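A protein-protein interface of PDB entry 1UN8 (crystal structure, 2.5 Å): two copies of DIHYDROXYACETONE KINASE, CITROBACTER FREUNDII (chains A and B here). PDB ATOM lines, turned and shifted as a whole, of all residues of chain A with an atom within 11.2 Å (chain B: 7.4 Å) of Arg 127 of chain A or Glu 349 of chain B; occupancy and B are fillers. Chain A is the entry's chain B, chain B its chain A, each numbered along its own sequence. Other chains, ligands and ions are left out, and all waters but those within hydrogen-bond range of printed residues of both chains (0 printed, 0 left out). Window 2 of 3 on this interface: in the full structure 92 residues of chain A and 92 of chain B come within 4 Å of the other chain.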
ATOM      1  N   LEU A  92      -0.206  28.378   1.833  1.00  0.00           N
ATOM      2  CA  LEU A  92      -0.841  27.069   1.910  1.00  0.00           C
ATOM      3  C   LEU A  92      -0.366  26.363   3.177  1.00  0.00           C
ATOM      4  O   LEU A  92      -1.180  25.913   4.000  1.00  0.00           O
ATOM      5  CB  LEU A  92      -0.502  26.232   0.667  1.00  0.00           C
ATOM      6  CG  LEU A  92      -1.179  24.858   0.580  1.00  0.00           C
ATOM      7  CD1 LEU A  92      -2.682  25.021   0.750  1.00  0.00           C
ATOM      8  CD2 LEU A  92      -0.848  24.191  -0.751  1.00  0.00           C
ATOM      9  N   ILE A  95      -2.165  27.333   6.170  1.00  0.00           N
ATOM     10  CA  ILE A  95      -3.541  26.854   6.181  1.00  0.00           C
ATOM     11  C   ILE A  95      -3.588  25.409   6.698  1.00  0.00           C
ATOM     12  O   ILE A  95      -4.301  25.085   7.656  1.00  0.00           O
ATOM     13  CB  ILE A  95      -4.166  26.924   4.750  1.00  0.00           C
ATOM     14  CG1 ILE A  95      -4.650  28.350   4.440  1.00  0.00           C
ATOM     15  CG2 ILE A  95      -5.356  25.965   4.652  1.00  0.00           C
ATOM     16  CD1 ILE A  95      -3.663  29.447   4.788  1.00  0.00           C
ATOM     17  N   GLN A  96      -2.811  24.547   6.055  1.00  0.00           N
ATOM     18  CA  GLN A  96      -2.745  23.142   6.422  1.00  0.00           C
ATOM     19  C   GLN A  96      -2.232  22.943   7.836  1.00  0.00           C
ATOM     20  O   GLN A  96      -2.589  21.965   8.504  1.00  0.00           O
ATOM     21  CB  GLN A  96      -1.809  22.397   5.486  1.00  0.00           C
ATOM     22  CG  GLN A  96      -2.231  22.403   4.053  1.00  0.00           C
ATOM     23  CD  GLN A  96      -1.762  21.160   3.343  1.00  0.00           C
ATOM     24  OE1 GLN A  96      -2.307  20.069   3.560  1.00  0.00           O
ATOM     25  NE2 GLN A  96      -0.735  21.301   2.502  1.00  0.00           N
ATOM     26  N   PHE A 118      -2.383  34.632  -1.800  1.00  0.00           N
ATOM     27  CA  PHE A 118      -3.232  34.001  -0.811  1.00  0.00           C
ATOM     28  C   PHE A 118      -4.366  33.339  -1.594  1.00  0.00           C
ATOM     29  O   PHE A 118      -4.863  32.278  -1.213  1.00  0.00           O
ATOM     30  CB  PHE A 118      -3.810  35.026   0.166  1.00  0.00           C
ATOM     31  CG  PHE A 118      -2.855  35.452   1.253  1.00  0.00           C
ATOM     32  CD1 PHE A 118      -1.807  36.331   0.984  1.00  0.00           C
ATOM     33  CD2 PHE A 118      -3.016  34.984   2.559  1.00  0.00           C
ATOM     34  CE1 PHE A 118      -0.937  36.741   1.998  1.00  0.00           C
ATOM     35  CE2 PHE A 118      -2.152  35.387   3.581  1.00  0.00           C
ATOM     36  CZ  PHE A 118      -1.114  36.265   3.302  1.00  0.00           C
ATOM     37  N   GLY A 119      -4.753  33.965  -2.709  1.00  0.00           N
ATOM     38  CA  GLY A 119      -5.819  33.437  -3.539  1.00  0.00           C
ATOM     39  C   GLY A 119      -5.531  32.059  -4.106  1.00  0.00           C
ATOM     40  O   GLY A 119      -6.317  31.123  -3.916  1.00  0.00           O
ATOM     41  N   LEU A 120      -4.417  31.922  -4.819  1.00  0.00           N
ATOM     42  CA  LEU A 120      -4.076  30.617  -5.369  1.00  0.00           C
ATOM     43  C   LEU A 120      -3.956  29.625  -4.211  1.00  0.00           C
ATOM     44  O   LEU A 120      -4.305  28.455  -4.354  1.00  0.00           O
ATOM     45  CB  LEU A 120      -2.763  30.675  -6.163  1.00  0.00           C
ATOM     46  CG  LEU A 120      -2.303  29.345  -6.769  1.00  0.00           C
ATOM     47  CD1 LEU A 120      -3.483  28.626  -7.426  1.00  0.00           C
ATOM     48  CD2 LEU A 120      -1.187  29.600  -7.783  1.00  0.00           C
ATOM     49  N   ALA A 121      -3.482  30.100  -3.059  1.00  0.00           N
ATOM     50  CA  ALA A 121      -3.345  29.246  -1.884  1.00  0.00           C
ATOM     51  C   ALA A 121      -4.717  28.727  -1.436  1.00  0.00           C
ATOM     52  O   ALA A 121      -4.884  27.524  -1.202  1.00  0.00           O
ATOM     53  CB  ALA A 121      -2.681  30.009  -0.746  1.00  0.00           C
ATOM     54  N   ALA A 122      -5.693  29.629  -1.318  1.00  0.00           N
ATOM     55  CA  ALA A 122      -7.040  29.245  -0.906  1.00  0.00           C
ATOM     56  C   ALA A 122      -7.589  28.196  -1.870  1.00  0.00           C
ATOM     57  O   ALA A 122      -8.207  27.211  -1.455  1.00  0.00           O
ATOM     58  CB  ALA A 122      -7.952  30.456  -0.893  1.00  0.00           C
ATOM     59  N   GLU A 123      -7.355  28.409  -3.161  1.00  0.00           N
ATOM     60  CA  GLU A 123      -7.824  27.484  -4.175  1.00  0.00           C
ATOM     61  C   GLU A 123      -7.191  26.114  -4.011  1.00  0.00           C
ATOM     62  O   GLU A 123      -7.876  25.099  -4.105  1.00  0.00           O
ATOM     63  CB  GLU A 123      -7.514  28.029  -5.567  1.00  0.00           C
ATOM     64  CG  GLU A 123      -8.247  29.304  -5.852  1.00  0.00           C
ATOM     65  CD  GLU A 123      -9.748  29.121  -5.782  1.00  0.00           C
ATOM     66  OE1 GLU A 123     -10.445  30.093  -5.405  1.00  0.00           O
ATOM     67  OE2 GLU A 123     -10.223  28.009  -6.115  1.00  0.00           O
ATOM     68  N   LYS A 124      -5.886  26.080  -3.775  1.00  0.00           N
ATOM     69  CA  LYS A 124      -5.201  24.802  -3.609  1.00  0.00           C
ATOM     70  C   LYS A 124      -5.646  24.141  -2.314  1.00  0.00           C
ATOM     71  O   LYS A 124      -5.621  22.915  -2.193  1.00  0.00           O
ATOM     72  CB  LYS A 124      -3.685  24.995  -3.593  1.00  0.00           C
ATOM     73  CG  LYS A 124      -3.100  25.346  -4.942  1.00  0.00           C
ATOM     74  CD  LYS A 124      -1.589  25.206  -4.931  1.00  0.00           C
ATOM     75  CE  LYS A 124      -1.022  25.319  -6.344  1.00  0.00           C
ATOM     76  NZ  LYS A 124       0.432  25.018  -6.375  1.00  0.00           N
ATOM     77  N   ALA A 125      -6.060  24.958  -1.351  1.00  0.00           N
ATOM     78  CA  ALA A 125      -6.504  24.451  -0.061  1.00  0.00           C
ATOM     79  C   ALA A 125      -7.869  23.802  -0.214  1.00  0.00           C
ATOM     80  O   ALA A 125      -8.127  22.728   0.329  1.00  0.00           O
ATOM     81  CB  ALA A 125      -6.576  25.582   0.946  1.00  0.00           C
ATOM     82  N   ARG A 126      -8.742  24.470  -0.961  1.00  0.00           N
ATOM     83  CA  ARG A 126     -10.084  23.966  -1.203  1.00  0.00           C
ATOM     84  C   ARG A 126     -10.047  22.606  -1.898  1.00  0.00           C
ATOM     85  O   ARG A 126     -10.854  21.728  -1.589  1.00  0.00           O
ATOM     86  CB  ARG A 126     -10.879  24.978  -2.028  1.00  0.00           C
ATOM     87  CG  ARG A 126     -11.357  26.156  -1.201  1.00  0.00           C
ATOM     88  CD  ARG A 126     -12.010  27.228  -2.049  1.00  0.00           C
ATOM     89  NE  ARG A 126     -12.590  28.271  -1.212  1.00  0.00           N
ATOM     90  CZ  ARG A 126     -12.913  29.484  -1.645  1.00  0.00           C
ATOM     91  NH1 ARG A 126     -12.702  29.807  -2.917  1.00  0.00           N
ATOM     92  NH2 ARG A 126     -13.452  30.366  -0.808  1.00  0.00           N
ATOM     93  N   ARG A 127      -9.111  22.426  -2.820  1.00  0.00           N
ATOM     94  CA  ARG A 127      -8.992  21.152  -3.503  1.00  0.00           C
ATOM     95  C   ARG A 127      -8.594  20.060  -2.501  1.00  0.00           C
ATOM     96  O   ARG A 127      -8.858  18.876  -2.715  1.00  0.00           O
ATOM     97  CB  ARG A 127      -7.950  21.236  -4.619  1.00  0.00           C
ATOM     98  CG  ARG A 127      -7.627  19.884  -5.225  1.00  0.00           C
ATOM     99  CD  ARG A 127      -6.674  19.998  -6.385  1.00  0.00           C
ATOM    100  NE  ARG A 127      -6.190  18.686  -6.800  1.00  0.00           N
ATOM    101  CZ  ARG A 127      -5.295  17.971  -6.121  1.00  0.00           C
ATOM    102  NH1 ARG A 127      -4.772  18.439  -4.987  1.00  0.00           N
ATOM    103  NH2 ARG A 127      -4.922  16.780  -6.576  1.00  0.00           N
ATOM    104  N   LEU A 128      -7.959  20.468  -1.407  1.00  0.00           N
ATOM    105  CA  LEU A 128      -7.528  19.541  -0.371  1.00  0.00           C
ATOM    106  C   LEU A 128      -8.603  19.359   0.708  1.00  0.00           C
ATOM    107  O   LEU A 128      -8.352  18.791   1.770  1.00  0.00           O
ATOM    108  CB  LEU A 128      -6.217  20.038   0.255  1.00  0.00           C
ATOM    109  CG  LEU A 128      -5.007  20.062  -0.691  1.00  0.00           C
ATOM    110  CD1 LEU A 128      -3.820  20.740  -0.019  1.00  0.00           C
ATOM    111  CD2 LEU A 128      -4.651  18.639  -1.100  1.00  0.00           C
ATOM    112  N   GLY A 129      -9.803  19.861   0.445  1.00  0.00           N
ATOM    113  CA  GLY A 129     -10.875  19.686   1.402  1.00  0.00           C
ATOM    114  C   GLY A 129     -11.039  20.706   2.507  1.00  0.00           C
ATOM    115  O   GLY A 129     -12.012  20.634   3.268  1.00  0.00           O
ATOM    116  N   TYR A 130     -10.114  21.653   2.623  1.00  0.00           N
ATOM    117  CA  TYR A 130     -10.248  22.657   3.669  1.00  0.00           C
ATOM    118  C   TYR A 130     -11.332  23.660   3.296  1.00  0.00           C
ATOM    119  O   TYR A 130     -11.580  23.905   2.115  1.00  0.00           O
ATOM    120  CB  TYR A 130      -8.937  23.414   3.876  1.00  0.00           C
ATOM    121  CG  TYR A 130      -7.756  22.573   4.306  1.00  0.00           C
ATOM    122  CD1 TYR A 130      -6.917  21.996   3.361  1.00  0.00           C
ATOM    123  CD2 TYR A 130      -7.460  22.384   5.659  1.00  0.00           C
ATOM    124  CE1 TYR A 130      -5.801  21.256   3.747  1.00  0.00           C
ATOM    125  CE2 TYR A 130      -6.350  21.645   6.061  1.00  0.00           C
ATOM    126  CZ  TYR A 130      -5.519  21.080   5.098  1.00  0.00           C
ATOM    127  OH  TYR A 130      -4.411  20.343   5.470  1.00  0.00           O
ATOM    128  N   ASN A 131     -11.993  24.219   4.307  1.00  0.00           N
ATOM    129  CA  ASN A 131     -13.013  25.229   4.076  1.00  0.00           C
ATOM    130  C   ASN A 131     -12.297  26.553   4.249  1.00  0.00           C
ATOM    131  O   ASN A 131     -11.766  26.840   5.324  1.00  0.00           O
ATOM    132  CB  ASN A 131     -14.150  25.118   5.088  1.00  0.00           C
ATOM    133  CG  ASN A 131     -15.073  23.950   4.794  1.00  0.00           C
ATOM    134  OD1 ASN A 131     -16.243  23.958   5.185  1.00  0.00           O
ATOM    135  ND2 ASN A 131     -14.551  22.933   4.107  1.00  0.00           N
ATOM    136  N   VAL A 132     -12.278  27.355   3.186  1.00  0.00           N
ATOM    137  CA  VAL A 132     -11.584  28.631   3.221  1.00  0.00           C
ATOM    138  C   VAL A 132     -12.401  29.814   2.722  1.00  0.00           C
ATOM    139  O   VAL A 132     -13.187  29.692   1.783  1.00  0.00           O
ATOM    140  CB  VAL A 132     -10.294  28.570   2.368  1.00  0.00           C
ATOM    141  CG1 VAL A 132      -9.412  29.772   2.669  1.00  0.00           C
ATOM    142  CG2 VAL A 132      -9.551  27.273   2.638  1.00  0.00           C
ATOM    143  N   GLU A 133     -12.199  30.956   3.365  1.00  0.00           N
ATOM    144  CA  GLU A 133     -12.857  32.193   2.969  1.00  0.00           C
ATOM    145  C   GLU A 133     -11.791  33.288   2.986  1.00  0.00           C
ATOM    146  O   GLU A 133     -10.858  33.234   3.792  1.00  0.00           O
ATOM    147  CB  GLU A 133     -13.988  32.552   3.927  1.00  0.00           C
ATOM    148  CG  GLU A 133     -15.227  31.667   3.801  1.00  0.00           C
ATOM    149  CD  GLU A 133     -15.767  31.572   2.371  1.00  0.00           C
ATOM    150  OE1 GLU A 133     -15.638  32.553   1.609  1.00  0.00           O
ATOM    151  OE2 GLU A 133     -16.337  30.516   2.016  1.00  0.00           O
ATOM    152  N   SER B 345       0.708  16.219   0.957  1.00  0.00           N
ATOM    153  CA  SER B 345       1.383  16.642  -0.267  1.00  0.00           C
ATOM    154  C   SER B 345       0.450  17.446  -1.162  1.00  0.00           C
ATOM    155  O   SER B 345      -0.577  16.941  -1.621  1.00  0.00           O
ATOM    156  CB  SER B 345       1.897  15.426  -1.043  1.00  0.00           C
ATOM    157  OG  SER B 345       2.457  15.823  -2.285  1.00  0.00           O
ATOM    158  N   ALA B 346       0.808  18.700  -1.407  1.00  0.00           N
ATOM    159  CA  ALA B 346      -0.006  19.554  -2.258  1.00  0.00           C
ATOM    160  C   ALA B 346      -0.036  18.952  -3.661  1.00  0.00           C
ATOM    161  O   ALA B 346      -1.074  18.952  -4.324  1.00  0.00           O
ATOM    162  CB  ALA B 346       0.580  20.962  -2.294  1.00  0.00           C
ATOM    163  N   ARG B 347       1.110  18.429  -4.092  1.00  0.00           N
ATOM    164  CA  ARG B 347       1.258  17.820  -5.409  1.00  0.00           C
ATOM    165  C   ARG B 347       0.040  17.006  -5.838  1.00  0.00           C
ATOM    166  O   ARG B 347      -0.390  16.093  -5.143  1.00  0.00           O
ATOM    167  CB  ARG B 347       2.510  16.939  -5.423  1.00  0.00           C
ATOM    168  CG  ARG B 347       2.604  15.968  -6.583  1.00  0.00           C
ATOM    169  CD  ARG B 347       3.737  14.989  -6.320  1.00  0.00           C
ATOM    170  NE  ARG B 347       3.445  13.658  -6.838  1.00  0.00           N
ATOM    171  CZ  ARG B 347       4.140  12.566  -6.518  1.00  0.00           C
ATOM    172  NH1 ARG B 347       5.170  12.655  -5.676  1.00  0.00           N
ATOM    173  NH2 ARG B 347       3.812  11.387  -7.032  1.00  0.00           N
ATOM    174  N   VAL B 348      -0.512  17.351  -6.995  1.00  0.00           N
ATOM    175  CA  VAL B 348      -1.676  16.658  -7.529  1.00  0.00           C
ATOM    176  C   VAL B 348      -1.282  15.321  -8.151  1.00  0.00           C
ATOM    177  O   VAL B 348      -0.304  15.223  -8.901  1.00  0.00           O
ATOM    178  CB  VAL B 348      -2.415  17.530  -8.591  1.00  0.00           C
ATOM    179  CG1 VAL B 348      -1.423  18.085  -9.597  1.00  0.00           C
ATOM    180  CG2 VAL B 348      -3.472  16.703  -9.308  1.00  0.00           C
ATOM    181  N   GLU B 349      -2.052  14.292  -7.820  1.00  0.00           N
ATOM    182  CA  GLU B 349      -1.814  12.950  -8.326  1.00  0.00           C
ATOM    183  C   GLU B 349      -2.624  12.689  -9.585  1.00  0.00           C
ATOM    184  O   GLU B 349      -3.723  13.220  -9.751  1.00  0.00           O
ATOM    185  CB  GLU B 349      -2.179  11.917  -7.270  1.00  0.00           C
ATOM    186  CG  GLU B 349      -1.122  11.706  -6.213  1.00  0.00           C
ATOM    187  CD  GLU B 349      -1.723  11.227  -4.907  1.00  0.00           C
ATOM    188  OE1 GLU B 349      -2.621  10.352  -4.947  1.00  0.00           O
ATOM    189  OE2 GLU B 349      -1.294  11.721  -3.841  1.00  0.00           O
ATOM    190  N   PHE B 350      -2.084  11.847 -10.461  1.00  0.00           N
ATOM    191  CA  PHE B 350      -2.749  11.536 -11.714  1.00  0.00           C
ATOM    192  C   PHE B 350      -2.075  10.370 -12.411  1.00  0.00           C
ATOM    193  O   PHE B 350      -0.960   9.976 -12.064  1.00  0.00           O
ATOM    194  CB  PHE B 350      -2.695  12.754 -12.635  1.00  0.00           C
ATOM    195  CG  PHE B 350      -1.306  13.095 -13.097  1.00  0.00           C
ATOM    196  CD1 PHE B 350      -0.835  12.646 -14.326  1.00  0.00           C
ATOM    197  CD2 PHE B 350      -0.458  13.851 -12.290  1.00  0.00           C
ATOM    198  CE1 PHE B 350       0.462  12.942 -14.750  1.00  0.00           C
ATOM    199  CE2 PHE B 350       0.842  14.154 -12.702  1.00  0.00           C
ATOM    200  CZ  PHE B 350       1.303  13.699 -13.935  1.00  0.00           C
ATOM    201  N   GLN B 351      -2.754   9.835 -13.417  1.00  0.00           N
ATOM    202  CA  GLN B 351      -2.219   8.728 -14.185  1.00  0.00           C
ATOM    203  C   GLN B 351      -2.446   9.029 -15.659  1.00  0.00           C
ATOM    204  O   GLN B 351      -3.575   9.276 -16.084  1.00  0.00           O
ATOM    205  CB  GLN B 351      -2.924   7.431 -13.796  1.00  0.00           C
ATOM    206  CG  GLN B 351      -2.043   6.200 -13.927  1.00  0.00           C
ATOM    207  CD  GLN B 351      -0.799   6.287 -13.050  1.00  0.00           C
ATOM    208  OE1 GLN B 351      -0.896   6.432 -11.830  1.00  0.00           O
ATOM    209  NE2 GLN B 351       0.376   6.204 -13.672  1.00  0.00           N
ATOM    210  N   PRO B 409      -3.207  13.351 -18.046  1.00  0.00           N
ATOM    211  CA  PRO B 409      -4.367  12.530 -17.687  1.00  0.00           C
ATOM    212  C   PRO B 409      -5.529  12.953 -18.581  1.00  0.00           C
ATOM    213  O   PRO B 409      -6.620  13.274 -18.100  1.00  0.00           O
ATOM    214  CB  PRO B 409      -4.604  12.904 -16.231  1.00  0.00           C
ATOM    215  CG  PRO B 409      -4.257  14.366 -16.225  1.00  0.00           C
ATOM    216  CD  PRO B 409      -2.975  14.403 -17.039  1.00  0.00           C
ATOM    217  N   ALA B 414     -11.090  17.010 -14.931  1.00  0.00           N
ATOM    218  CA  ALA B 414     -10.904  17.508 -13.569  1.00  0.00           C
ATOM    219  C   ALA B 414      -9.438  17.434 -13.155  1.00  0.00           C
ATOM    220  O   ALA B 414      -8.831  18.434 -12.787  1.00  0.00           O
ATOM    221  CB  ALA B 414     -11.760  16.710 -12.601  1.00  0.00           C
ATOM    222  N   THR B 415      -8.870  16.241 -13.232  1.00  0.00           N
ATOM    223  CA  THR B 415      -7.476  16.039 -12.868  1.00  0.00           C
ATOM    224  C   THR B 415      -6.557  16.749 -13.856  1.00  0.00           C
ATOM    225  O   THR B 415      -5.505  17.263 -13.470  1.00  0.00           O
ATOM    226  CB  THR B 415      -7.149  14.537 -12.824  1.00  0.00           C
ATOM    227  OG1 THR B 415      -8.082  13.887 -11.949  1.00  0.00           O
ATOM    228  CG2 THR B 415      -5.739  14.305 -12.299  1.00  0.00           C
ATOM    229  N   LEU B 416      -6.955  16.783 -15.125  1.00  0.00           N
ATOM    230  CA  LEU B 416      -6.154  17.461 -16.136  1.00  0.00           C
ATOM    231  C   LEU B 416      -6.038  18.933 -15.805  1.00  0.00           C
ATOM    232  O   LEU B 416      -4.940  19.485 -15.799  1.00  0.00           O
ATOM    233  CB  LEU B 416      -6.771  17.329 -17.526  1.00  0.00           C
ATOM    234  CG  LEU B 416      -5.986  18.111 -18.586  1.00  0.00           C
ATOM    235  CD1 LEU B 416      -4.588  17.505 -18.748  1.00  0.00           C
ATOM    236  CD2 LEU B 416      -6.738  18.092 -19.905  1.00  0.00           C
ATOM    237  N   ALA B 418      -6.590  20.391 -12.928  1.00  0.00           N
ATOM    238  CA  ALA B 418      -5.858  20.481 -11.673  1.00  0.00           C
ATOM    239  C   ALA B 418      -4.353  20.367 -11.928  1.00  0.00           C
ATOM    240  O   ALA B 418      -3.554  21.023 -11.266  1.00  0.00           O
ATOM    241  CB  ALA B 418      -6.316  19.379 -10.723  1.00  0.00           C
ATOM    242  N   LEU B 419      -3.970  19.540 -12.894  1.00  0.00           N
ATOM    243  CA  LEU B 419      -2.556  19.368 -13.202  1.00  0.00           C
ATOM    244  C   LEU B 419      -1.970  20.604 -13.878  1.00  0.00           C
ATOM    245  O   LEU B 419      -0.851  21.019 -13.568  1.00  0.00           O
ATOM    246  CB  LEU B 419      -2.350  18.148 -14.096  1.00  0.00           C
ATOM    247  CG  LEU B 419      -0.885  17.967 -14.497  1.00  0.00           C
ATOM    248  CD1 LEU B 419      -0.032  17.798 -13.243  1.00  0.00           C
ATOM    249  CD2 LEU B 419      -0.753  16.767 -15.419  1.00  0.00           C
ATOM    250  N   GLU B 422      -1.549  23.370 -11.495  1.00  0.00           N
ATOM    251  CA  GLU B 422      -0.379  23.188 -10.662  1.00  0.00           C
ATOM    252  C   GLU B 422       0.909  23.534 -11.391  1.00  0.00           C
ATOM    253  O   GLU B 422       1.815  24.120 -10.815  1.00  0.00           O
ATOM    254  CB  GLU B 422      -0.307  21.741 -10.185  1.00  0.00           C
ATOM    255  CG  GLU B 422       0.802  21.470  -9.179  1.00  0.00           C
ATOM    256  CD  GLU B 422       1.082  19.982  -9.008  1.00  0.00           C
ATOM    257  OE1 GLU B 422       1.701  19.375  -9.916  1.00  0.00           O
ATOM    258  OE2 GLU B 422       0.674  19.421  -7.966  1.00  0.00           O
ATOM    259  N   THR B 441      -7.131  25.798 -11.567  1.00  0.00           N
ATOM    260  CA  THR B 441      -7.300  25.125 -10.284  1.00  0.00           C
ATOM    261  C   THR B 441      -8.767  25.152  -9.881  1.00  0.00           C
ATOM    262  O   THR B 441      -9.346  24.121  -9.538  1.00  0.00           O
ATOM    263  CB  THR B 441      -6.458  25.798  -9.185  1.00  0.00           C
ATOM    264  OG1 THR B 441      -5.075  25.736  -9.555  1.00  0.00           O
ATOM    265  CG2 THR B 441      -6.643  25.094  -7.851  1.00  0.00           C
ATOM    266  N   GLY B 444     -10.774  23.099 -12.416  1.00  0.00           N
ATOM    267  CA  GLY B 444     -10.603  21.680 -12.179  1.00  0.00           C
ATOM    268  C   GLY B 444     -11.460  21.216 -11.024  1.00  0.00           C
ATOM    269  O   GLY B 444     -11.960  20.096 -11.030  1.00  0.00           O
ATOM    270  N   GLN B 445     -11.634  22.082 -10.034  1.00  0.00           N
ATOM    271  CA  GLN B 445     -12.433  21.750  -8.868  1.00  0.00           C
ATOM    272  C   GLN B 445     -13.927  21.819  -9.134  1.00  0.00           C
ATOM    273  O   GLN B 445     -14.705  21.082  -8.530  1.00  0.00           O
ATOM    274  CB  GLN B 445     -12.068  22.667  -7.705  1.00  0.00           C
ATOM    275  CG  GLN B 445     -10.933  22.116  -6.868  1.00  0.00           C
ATOM    276  CD  GLN B 445     -11.300  20.789  -6.245  1.00  0.00           C
ATOM    277  OE1 GLN B 445     -12.171  20.732  -5.372  1.00  0.00           O
ATOM    278  NE2 GLN B 445     -10.652  19.711  -6.699  1.00  0.00           N
ATOM    279  N   GLU B 448     -14.675  18.673 -10.640  1.00  0.00           N
ATOM    280  CA  GLU B 448     -14.661  17.607  -9.644  1.00  0.00           C
ATOM    281  C   GLU B 448     -16.028  17.508  -8.976  1.00  0.00           C
ATOM    282  O   GLU B 448     -16.431  16.437  -8.523  1.00  0.00           O
ATOM    283  CB  GLU B 448     -13.587  17.866  -8.590  1.00  0.00           C
ATOM    284  CG  GLU B 448     -13.097  16.597  -7.937  1.00  0.00           C
ATOM    285  CD  GLU B 448     -12.410  15.683  -8.933  1.00  0.00           C
ATOM    286  OE1 GLU B 448     -11.337  16.072  -9.448  1.00  0.00           O
ATOM    287  OE2 GLU B 448     -12.940  14.581  -9.204  1.00  0.00           O
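NH1 of Arg 126 of chain A lies within salt-bridge range of OE1 of Glu 123 of chain A, 3.4 Å away.
The backbone NH (N) of Val 348 of chain B lies within hydrogen-bond range of the side-chain carboxylate (OE2) of Glu 422 of chain B (2.6 Å).
Leu 92 of chain A touches Ala 346 of chain B.
Leu 120 of chain A touches Thr 441 of chain B (CD1 to OG1, 3.9 Å).
Glu 123 of chain A touches Thr 441 of chain B.
Ala 346 of chain B touches Arg 127 of chain A (O to NH1, 3.8 Å).
Arg 127 of chain A touches Val 348 of chain B (NH2 to CG2, 3.1 Å).
Glu 349 of chain B touches Arg 127 of chain A.
Arg 127 of chain A touches Ala 418 of chain B.
Gln 445 of chain B touches Arg 127 of chain A (NE2 to CG, 3.4 Å).
Printed residues of chain B within 4 Å of Arg 127 of chain A: Ala 346 (3.8 Å), Val 348 (3.1 Å), Glu 349 (3.997 Å), Ala 418 (3.99 Å) and Gln 445 (3.4 Å).
Of the printed residues of chain A, Glu 349 of chain B touches Arg 127 (3.997 Å).
No residue of chain A comes within 4 Å of Ser 345 of chain B.
Arg 347 of chain B touches none of the printed residues of chain A.
Val 348 of chain B touches just one residue of chain A: Arg 127.
No residue of chain A comes within 4 Å of Phe 350 of chain B.
Printed residues of chain A within 4 Å of Thr 441 of chain B: Leu 120 and Glu 123.
Of the printed residues of chain A, Gln 445 of chain B touches Arg 127.
Printed residues of chain B within 4 Å of Leu 120 of chain A: Thr 441.
Of the printed residues of chain B, Glu 123 of chain A touches Thr 441.
Leu 419 of chain B touches none of the printed residues of chain A.
Glu 133 of chain A touches none of the printed residues of chain B.
The nearest printed residue of chain A that does not touch Glu 349 of chain B is Leu 128 of chain A (8.2 Å).
Of the 19 printed residues of chain A, 4 touch a printed residue of chain B.
Printed residues of chain A that touch a printed residue of chain B: Leu 92, Leu 120, Glu 123 and Arg 127.
Hydrophobic or aromatic side chains of chain A that line the printed part of chain B: Leu 92 and Leu 120.
Printed residues of chain B that touch a printed residue of chain A: Ala 346, Val 348, Glu 349, Ala 418, Thr 441 and Gln 445.
Among the printed residues, no Asp or Glu carboxylate lies within 4 Å of a Lys or Arg side-chain nitrogen of the other chain.
No position is printed for both chains.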
